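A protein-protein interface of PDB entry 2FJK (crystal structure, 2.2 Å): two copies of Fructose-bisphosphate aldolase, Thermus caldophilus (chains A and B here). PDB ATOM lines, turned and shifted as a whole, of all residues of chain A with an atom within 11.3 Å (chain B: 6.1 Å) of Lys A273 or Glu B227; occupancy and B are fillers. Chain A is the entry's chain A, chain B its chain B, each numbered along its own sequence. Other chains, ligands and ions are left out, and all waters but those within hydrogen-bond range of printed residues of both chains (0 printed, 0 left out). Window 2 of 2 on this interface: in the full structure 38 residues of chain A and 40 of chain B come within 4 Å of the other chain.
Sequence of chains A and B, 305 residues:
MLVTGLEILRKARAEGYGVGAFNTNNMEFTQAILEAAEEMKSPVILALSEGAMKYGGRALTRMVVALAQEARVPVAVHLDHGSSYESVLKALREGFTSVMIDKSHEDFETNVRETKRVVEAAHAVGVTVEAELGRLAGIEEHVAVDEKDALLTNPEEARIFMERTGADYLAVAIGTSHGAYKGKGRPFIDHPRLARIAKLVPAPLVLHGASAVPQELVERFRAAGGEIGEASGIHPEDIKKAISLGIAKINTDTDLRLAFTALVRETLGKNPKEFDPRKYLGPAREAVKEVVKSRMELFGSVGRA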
ATOM      1  N   VAL A 264      33.944  27.273  -7.837  1.00  0.00           N
ATOM      2  CA  VAL A 264      32.963  26.468  -7.123  1.00  0.00           C
ATOM      3  C   VAL A 264      33.066  26.776  -5.630  1.00  0.00           C
ATOM      4  O   VAL A 264      32.054  26.999  -4.959  1.00  0.00           O
ATOM      5  CB  VAL A 264      33.187  24.948  -7.337  1.00  0.00           C
ATOM      6  CG1 VAL A 264      32.388  24.158  -6.314  1.00  0.00           C
ATOM      7  CG2 VAL A 264      32.752  24.543  -8.741  1.00  0.00           C
ATOM      8  N   ARG A 265      34.296  26.802  -5.121  1.00  0.00           N
ATOM      9  CA  ARG A 265      34.528  27.080  -3.708  1.00  0.00           C
ATOM     10  C   ARG A 265      34.002  28.444  -3.288  1.00  0.00           C
ATOM     11  O   ARG A 265      33.283  28.553  -2.297  1.00  0.00           O
ATOM     12  CB  ARG A 265      36.029  27.003  -3.365  1.00  0.00           C
ATOM     13  CG  ARG A 265      36.683  25.659  -3.655  1.00  0.00           C
ATOM     14  CD  ARG A 265      38.008  25.517  -2.932  1.00  0.00           C
ATOM     15  NE  ARG A 265      37.813  24.936  -1.610  1.00  0.00           N
ATOM     16  CZ  ARG A 265      38.153  23.692  -1.283  1.00  0.00           C
ATOM     17  NH1 ARG A 265      38.723  22.885  -2.180  1.00  0.00           N
ATOM     18  NH2 ARG A 265      37.902  23.248  -0.063  1.00  0.00           N
ATOM     19  N   GLU A 266      34.354  29.488  -4.034  1.00  0.00           N
ATOM     20  CA  GLU A 266      33.895  30.814  -3.653  1.00  0.00           C
ATOM     21  C   GLU A 266      32.385  31.022  -3.783  1.00  0.00           C
ATOM     22  O   GLU A 266      31.794  31.700  -2.946  1.00  0.00           O
ATOM     23  CB  GLU A 266      34.667  31.912  -4.413  1.00  0.00           C
ATOM     24  CG  GLU A 266      34.383  32.068  -5.888  1.00  0.00           C
ATOM     25  CD  GLU A 266      34.888  33.415  -6.436  1.00  0.00           C
ATOM     26  OE1 GLU A 266      36.053  33.783  -6.161  1.00  0.00           O
ATOM     27  OE2 GLU A 266      34.118  34.100  -7.144  1.00  0.00           O
ATOM     28  N   THR A 267      31.758  30.446  -4.811  1.00  0.00           N
ATOM     29  CA  THR A 267      30.311  30.598  -4.983  1.00  0.00           C
ATOM     30  C   THR A 267      29.586  29.915  -3.830  1.00  0.00           C
ATOM     31  O   THR A 267      28.663  30.480  -3.243  1.00  0.00           O
ATOM     32  CB  THR A 267      29.808  29.964  -6.303  1.00  0.00           C
ATOM     33  OG1 THR A 267      30.463  30.575  -7.422  1.00  0.00           O
ATOM     34  CG2 THR A 267      28.316  30.170  -6.449  1.00  0.00           C
ATOM     35  N   LEU A 268      30.016  28.695  -3.499  1.00  0.00           N
ATOM     36  CA  LEU A 268      29.402  27.942  -2.411  1.00  0.00           C
ATOM     37  C   LEU A 268      29.763  28.552  -1.060  1.00  0.00           C
ATOM     38  O   LEU A 268      28.985  28.474  -0.108  1.00  0.00           O
ATOM     39  CB  LEU A 268      29.840  26.474  -2.466  1.00  0.00           C
ATOM     40  CG  LEU A 268      29.240  25.623  -3.596  1.00  0.00           C
ATOM     41  CD1 LEU A 268      29.917  24.262  -3.594  1.00  0.00           C
ATOM     42  CD2 LEU A 268      27.723  25.462  -3.411  1.00  0.00           C
ATOM     43  N   GLY A 269      30.947  29.158  -0.979  1.00  0.00           N
ATOM     44  CA  GLY A 269      31.361  29.796   0.263  1.00  0.00           C
ATOM     45  C   GLY A 269      30.564  31.072   0.499  1.00  0.00           C
ATOM     46  O   GLY A 269      30.156  31.369   1.615  1.00  0.00           O
ATOM     47  N   LYS A 270      30.328  31.825  -0.567  1.00  0.00           N
ATOM     48  CA  LYS A 270      29.570  33.076  -0.484  1.00  0.00           C
ATOM     49  C   LYS A 270      28.059  32.897  -0.344  1.00  0.00           C
ATOM     50  O   LYS A 270      27.370  33.781   0.164  1.00  0.00           O
ATOM     51  CB  LYS A 270      29.795  33.915  -1.736  1.00  0.00           C
ATOM     52  CG  LYS A 270      31.195  34.435  -1.961  1.00  0.00           C
ATOM     53  CD  LYS A 270      31.207  35.173  -3.296  1.00  0.00           C
ATOM     54  CE  LYS A 270      32.449  36.014  -3.499  1.00  0.00           C
ATOM     55  NZ  LYS A 270      32.329  36.803  -4.762  1.00  0.00           N
ATOM     56  N   ASN A 271      27.537  31.774  -0.824  1.00  0.00           N
ATOM     57  CA  ASN A 271      26.101  31.544  -0.783  1.00  0.00           C
ATOM     58  C   ASN A 271      25.759  30.168  -0.256  1.00  0.00           C
ATOM     59  O   ASN A 271      25.410  29.268  -1.013  1.00  0.00           O
ATOM     60  CB  ASN A 271      25.524  31.710  -2.183  1.00  0.00           C
ATOM     61  CG  ASN A 271      25.954  33.005  -2.832  1.00  0.00           C
ATOM     62  OD1 ASN A 271      25.291  34.032  -2.693  1.00  0.00           O
ATOM     63  ND2 ASN A 271      27.084  32.969  -3.530  1.00  0.00           N
ATOM     64  N   PRO A 272      25.846  29.994   1.063  1.00  0.00           N
ATOM     65  CA  PRO A 272      25.543  28.716   1.703  1.00  0.00           C
ATOM     66  C   PRO A 272      24.133  28.198   1.408  1.00  0.00           C
ATOM     67  O   PRO A 272      23.889  27.001   1.487  1.00  0.00           O
ATOM     68  CB  PRO A 272      25.746  29.017   3.189  1.00  0.00           C
ATOM     69  CG  PRO A 272      26.770  30.109   3.196  1.00  0.00           C
ATOM     70  CD  PRO A 272      26.320  30.986   2.047  1.00  0.00           C
ATOM     71  N   LYS A 273      23.206  29.086   1.068  1.00  0.00           N
ATOM     72  CA  LYS A 273      21.835  28.653   0.790  1.00  0.00           C
ATOM     73  C   LYS A 273      21.674  28.071  -0.611  1.00  0.00           C
ATOM     74  O   LYS A 273      20.623  27.537  -0.953  1.00  0.00           O
ATOM     75  CB  LYS A 273      20.862  29.823   0.950  1.00  0.00           C
ATOM     76  CG  LYS A 273      20.839  30.450   2.340  1.00  0.00           C
ATOM     77  CD  LYS A 273      19.851  31.609   2.390  1.00  0.00           C
ATOM     78  CE  LYS A 273      19.910  32.341   3.726  1.00  0.00           C
ATOM     79  NZ  LYS A 273      19.754  31.409   4.886  1.00  0.00           N
ATOM     80  N   GLU A 274      22.725  28.165  -1.414  1.00  0.00           N
ATOM     81  CA  GLU A 274      22.679  27.694  -2.788  1.00  0.00           C
ATOM     82  C   GLU A 274      22.832  26.185  -2.995  1.00  0.00           C
ATOM     83  O   GLU A 274      23.781  25.571  -2.483  1.00  0.00           O
ATOM     84  CB  GLU A 274      23.759  28.411  -3.595  1.00  0.00           C
ATOM     85  CG  GLU A 274      23.694  28.126  -5.061  1.00  0.00           C
ATOM     86  CD  GLU A 274      22.443  28.698  -5.691  1.00  0.00           C
ATOM     87  OE1 GLU A 274      22.369  29.936  -5.829  1.00  0.00           O
ATOM     88  OE2 GLU A 274      21.533  27.912  -6.041  1.00  0.00           O
ATOM     89  N   PHE A 275      21.900  25.588  -3.742  1.00  0.00           N
ATOM     90  CA  PHE A 275      21.991  24.166  -4.061  1.00  0.00           C
ATOM     91  C   PHE A 275      21.617  23.837  -5.513  1.00  0.00           C
ATOM     92  O   PHE A 275      21.486  22.665  -5.883  1.00  0.00           O
ATOM     93  CB  PHE A 275      21.194  23.313  -3.064  1.00  0.00           C
ATOM     94  CG  PHE A 275      19.731  23.644  -2.982  1.00  0.00           C
ATOM     95  CD1 PHE A 275      18.850  23.204  -3.957  1.00  0.00           C
ATOM     96  CD2 PHE A 275      19.232  24.371  -1.901  1.00  0.00           C
ATOM     97  CE1 PHE A 275      17.485  23.478  -3.858  1.00  0.00           C
ATOM     98  CE2 PHE A 275      17.873  24.649  -1.796  1.00  0.00           C
ATOM     99  CZ  PHE A 275      16.999  24.202  -2.773  1.00  0.00           C
ATOM    100  N   ASP A 276      21.454  24.879  -6.328  1.00  0.00           N
ATOM    101  CA  ASP A 276      21.160  24.727  -7.753  1.00  0.00           C
ATOM    102  C   ASP A 276      22.553  24.621  -8.378  1.00  0.00           C
ATOM    103  O   ASP A 276      23.296  25.598  -8.415  1.00  0.00           O
ATOM    104  CB  ASP A 276      20.443  25.968  -8.300  1.00  0.00           C
ATOM    105  CG  ASP A 276      20.159  25.882  -9.802  1.00  0.00           C
ATOM    106  OD1 ASP A 276      20.852  25.127 -10.521  1.00  0.00           O
ATOM    107  OD2 ASP A 276      19.243  26.587 -10.273  1.00  0.00           O
ATOM    108  N   PRO A 277      22.924  23.426  -8.874  1.00  0.00           N
ATOM    109  CA  PRO A 277      24.233  23.195  -9.485  1.00  0.00           C
ATOM    110  C   PRO A 277      24.753  24.266 -10.450  1.00  0.00           C
ATOM    111  O   PRO A 277      25.882  24.742 -10.318  1.00  0.00           O
ATOM    112  CB  PRO A 277      24.057  21.844 -10.170  1.00  0.00           C
ATOM    113  CG  PRO A 277      23.131  21.126  -9.237  1.00  0.00           C
ATOM    114  CD  PRO A 277      22.100  22.203  -8.924  1.00  0.00           C
ATOM    115  N   LYS A 279      24.328  27.276 -10.612  1.00  0.00           N
ATOM    116  CA  LYS A 279      24.704  28.529  -9.965  1.00  0.00           C
ATOM    117  C   LYS A 279      26.191  28.529  -9.601  1.00  0.00           C
ATOM    118  O   LYS A 279      26.801  29.593  -9.490  1.00  0.00           O
ATOM    119  CB  LYS A 279      23.866  28.777  -8.705  1.00  0.00           C
ATOM    120  CG  LYS A 279      22.366  28.996  -8.957  1.00  0.00           C
ATOM    121  CD  LYS A 279      22.104  30.253  -9.777  1.00  0.00           C
ATOM    122  CE  LYS A 279      20.622  30.405 -10.075  1.00  0.00           C
ATOM    123  NZ  LYS A 279      20.357  31.413 -11.142  1.00  0.00           N
ATOM    124  N   TYR A 280      26.774  27.351  -9.386  1.00  0.00           N
ATOM    125  CA  TYR A 280      28.197  27.313  -9.081  1.00  0.00           C
ATOM    126  C   TYR A 280      29.028  26.680 -10.190  1.00  0.00           C
ATOM    127  O   TYR A 280      30.211  26.998 -10.338  1.00  0.00           O
ATOM    128  CB  TYR A 280      28.479  26.659  -7.709  1.00  0.00           C
ATOM    129  CG  TYR A 280      27.854  25.303  -7.413  1.00  0.00           C
ATOM    130  CD1 TYR A 280      28.471  24.123  -7.819  1.00  0.00           C
ATOM    131  CD2 TYR A 280      26.669  25.208  -6.682  1.00  0.00           C
ATOM    132  CE1 TYR A 280      27.926  22.868  -7.500  1.00  0.00           C
ATOM    133  CE2 TYR A 280      26.112  23.969  -6.363  1.00  0.00           C
ATOM    134  CZ  TYR A 280      26.745  22.800  -6.774  1.00  0.00           C
ATOM    135  OH  TYR A 280      26.188  21.573  -6.469  1.00  0.00           O
ATOM    136  N   TYR B 181      10.307  24.481  -0.080  1.00  0.00           N
ATOM    137  CA  TYR B 181       9.322  24.880   0.934  1.00  0.00           C
ATOM    138  C   TYR B 181       7.903  24.699   0.414  1.00  0.00           C
ATOM    139  O   TYR B 181       7.231  25.670   0.046  1.00  0.00           O
ATOM    140  CB  TYR B 181       9.533  26.342   1.344  1.00  0.00           C
ATOM    141  CG  TYR B 181      10.944  26.622   1.799  1.00  0.00           C
ATOM    142  CD1 TYR B 181      11.899  27.094   0.906  1.00  0.00           C
ATOM    143  CD2 TYR B 181      11.340  26.360   3.110  1.00  0.00           C
ATOM    144  CE1 TYR B 181      13.211  27.300   1.300  1.00  0.00           C
ATOM    145  CE2 TYR B 181      12.651  26.559   3.517  1.00  0.00           C
ATOM    146  CZ  TYR B 181      13.583  27.031   2.605  1.00  0.00           C
ATOM    147  OH  TYR B 181      14.882  27.245   2.992  1.00  0.00           O
ATOM    148  N   PHE B 221      22.910  18.541   4.243  1.00  0.00           N
ATOM    149  CA  PHE B 221      23.239  19.816   3.611  1.00  0.00           C
ATOM    150  C   PHE B 221      23.767  20.763   4.689  1.00  0.00           C
ATOM    151  O   PHE B 221      24.844  21.346   4.541  1.00  0.00           O
ATOM    152  CB  PHE B 221      21.992  20.407   2.948  1.00  0.00           C
ATOM    153  CG  PHE B 221      22.259  21.632   2.120  1.00  0.00           C
ATOM    154  CD1 PHE B 221      23.105  21.574   1.020  1.00  0.00           C
ATOM    155  CD2 PHE B 221      21.630  22.836   2.415  1.00  0.00           C
ATOM    156  CE1 PHE B 221      23.322  22.700   0.222  1.00  0.00           C
ATOM    157  CE2 PHE B 221      21.838  23.971   1.623  1.00  0.00           C
ATOM    158  CZ  PHE B 221      22.684  23.901   0.525  1.00  0.00           C
ATOM    159  N   ARG B 222      23.020  20.907   5.780  1.00  0.00           N
ATOM    160  CA  ARG B 222      23.461  21.771   6.869  1.00  0.00           C
ATOM    161  C   ARG B 222      24.812  21.344   7.440  1.00  0.00           C
ATOM    162  O   ARG B 222      25.709  22.177   7.606  1.00  0.00           O
ATOM    163  CB  ARG B 222      22.437  21.797   8.000  1.00  0.00           C
ATOM    164  CG  ARG B 222      21.143  22.484   7.654  1.00  0.00           C
ATOM    165  CD  ARG B 222      20.496  23.077   8.904  1.00  0.00           C
ATOM    166  NE  ARG B 222      19.132  23.527   8.644  1.00  0.00           N
ATOM    167  CZ  ARG B 222      18.055  22.758   8.772  1.00  0.00           C
ATOM    168  NH1 ARG B 222      18.182  21.498   9.168  1.00  0.00           N
ATOM    169  NH2 ARG B 222      16.855  23.247   8.495  1.00  0.00           N
ATOM    170  N   GLY B 225      28.038  22.383   3.832  1.00  0.00           N
ATOM    171  CA  GLY B 225      27.855  23.807   3.578  1.00  0.00           C
ATOM    172  C   GLY B 225      26.758  24.481   4.407  1.00  0.00           C
ATOM    173  O   GLY B 225      26.934  25.606   4.873  1.00  0.00           O
ATOM    174  N   GLY B 226      25.618  23.810   4.557  1.00  0.00           N
ATOM    175  CA  GLY B 226      24.527  24.347   5.357  1.00  0.00           C
ATOM    176  C   GLY B 226      23.665  25.456   4.789  1.00  0.00           C
ATOM    177  O   GLY B 226      23.699  25.747   3.598  1.00  0.00           O
ATOM    178  N   GLU B 227      22.883  26.073   5.673  1.00  0.00           N
ATOM    179  CA  GLU B 227      21.970  27.171   5.341  1.00  0.00           C
ATOM    180  C   GLU B 227      20.722  26.738   4.584  1.00  0.00           C
ATOM    181  O   GLU B 227      20.687  26.743   3.355  1.00  0.00           O
ATOM    182  CB  GLU B 227      22.685  28.263   4.543  1.00  0.00           C
ATOM    183  CG  GLU B 227      23.662  29.109   5.345  1.00  0.00           C
ATOM    184  CD  GLU B 227      22.994  30.040   6.339  1.00  0.00           C
ATOM    185  OE1 GLU B 227      21.903  30.567   6.032  1.00  0.00           O
ATOM    186  OE2 GLU B 227      23.580  30.254   7.422  1.00  0.00           O
ATOM    187  N   ILE B 228      19.695  26.378   5.342  1.00  0.00           N
ATOM    188  CA  ILE B 228      18.414  25.953   4.796  1.00  0.00           C
ATOM    189  C   ILE B 228      17.395  26.112   5.917  1.00  0.00           C
ATOM    190  O   ILE B 228      17.698  25.840   7.080  1.00  0.00           O
ATOM    191  CB  ILE B 228      18.456  24.467   4.325  1.00  0.00           C
ATOM    192  CG1 ILE B 228      17.105  24.060   3.735  1.00  0.00           C
ATOM    193  CG2 ILE B 228      18.790  23.550   5.488  1.00  0.00           C
ATOM    194  CD1 ILE B 228      16.658  24.916   2.588  1.00  0.00           C
ATOM    195  N   GLY B 229      16.192  26.558   5.569  1.00  0.00           N
ATOM    196  CA  GLY B 229      15.162  26.754   6.575  1.00  0.00           C
ATOM    197  C   GLY B 229      14.319  25.535   6.894  1.00  0.00           C
ATOM    198  O   GLY B 229      14.796  24.399   6.844  1.00  0.00           O
ATOM    199  N   ARG B 265      29.759  20.050  -1.290  1.00  0.00           N
ATOM    200  CA  ARG B 265      30.211  20.817  -0.136  1.00  0.00           C
ATOM    201  C   ARG B 265      30.998  19.971   0.853  1.00  0.00           C
ATOM    202  O   ARG B 265      32.072  20.382   1.289  1.00  0.00           O
ATOM    203  CB  ARG B 265      29.025  21.490   0.576  1.00  0.00           C
ATOM    204  CG  ARG B 265      28.110  22.246  -0.360  1.00  0.00           C
ATOM    205  CD  ARG B 265      27.056  23.032   0.375  1.00  0.00           C
ATOM    206  NE  ARG B 265      27.600  24.286   0.871  1.00  0.00           N
ATOM    207  CZ  ARG B 265      27.124  25.483   0.549  1.00  0.00           C
ATOM    208  NH1 ARG B 265      26.078  25.599  -0.276  1.00  0.00           N
ATOM    209  NH2 ARG B 265      27.702  26.565   1.047  1.00  0.00           N
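Asn A271 touches Arg B265 (O to NH1, 3.8 Å).
Pro A272 touches Phe B221.
Gly B225 touches Pro A272 (O to CB, 3.99 Å).
Pro A272 touches Glu B227 (CB to CG, 3.0 Å).
CZ of Phe B221 touches O of Glu A274, 3.6 Å away.
Phe A275 touches Phe B221.
1 position is printed for both chains.
Of the 11 pairs that touch across the chains among the printed residues, none has its exchanged pair printed and touching as well.
The side-chain carboxylate (OE2) of Glu A274 lies within hydrogen-bond range of the backbone NH (N) of Asp A276 (3.0 Å).
The backbone carbonyl oxygen (O) of Phe B221 is in hydrogen-bond range of the backbone NH (N) of Gly B226, 2.6 Å away.
The backbone carbonyl oxygen (O) of Thr A267 is in hydrogen-bond range of the side-chain amide nitrogen (ND2) of Asn A271 (3.0 Å).
Of the 16 printed residues of chain A, 6 touch a printed residue of chain B.
Hydrophobic or aromatic side chains of chain A that line the printed part of chain B: Leu A268, Pro A272 and Phe A275.
Of the 9 printed residues of chain B, 5 touch a printed residue of chain A.
Hydrophobic or aromatic side chains of chain B that line the printed part of chain A: Phe B221.
Among the printed residues, Asp or Glu carboxylates within 4 Å of a Lys or Arg side-chain nitrogen of the other chain: Lys A273 with Glu B227.
Of the printed residues of chain B, Leu A268 touches Arg B265.
Of the printed residues of chain B, Asn A271 touches Arg B265.
Of chain B, only Glu B227 comes within 4 Å of Lys A273.
Printed residues of chain B within 4 Å of Phe A275: Phe B221 (3.9 Å).
Printed residues of chain A within 4 Å of Phe B221: Pro A272, Glu A274 and Phe A275.
Of chain A, only Pro A272 comes within 4 Å of Gly B226.
No residue of chain A comes within 4 Å of Ile B228.
No residue of chain A comes within 4 Å of Gly B229.
Printed residues of chain A within 4 Å of Arg B265: Leu A268 (2.6 Å), Asn A271 (3.8 Å), Pro A272 (3.1 Å) and Glu A274 (3.2 Å).
The nearest residue of chain B that does not touch Lys A273 is Gly B226 (4.2 Å).
O of Pro A272 is in hydrogen-bond range of NH1 of Arg B265, at 3.1 Å.
O of Leu A268 is in hydrogen-bond range of NH2 of Arg B265 (2.6 Å).
O of Glu A274 sits at hydrogen-bond distance from NH1 of Arg B265, 3.2 Å away.
O of Pro A272 sits close to O of Gly B226, at 2.5 Å.
The side-chain amino group (NZ) of Lys A273 lies within salt-bridge range of the side-chain carboxylate (OE1) of Glu B227 (2.6 Å).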
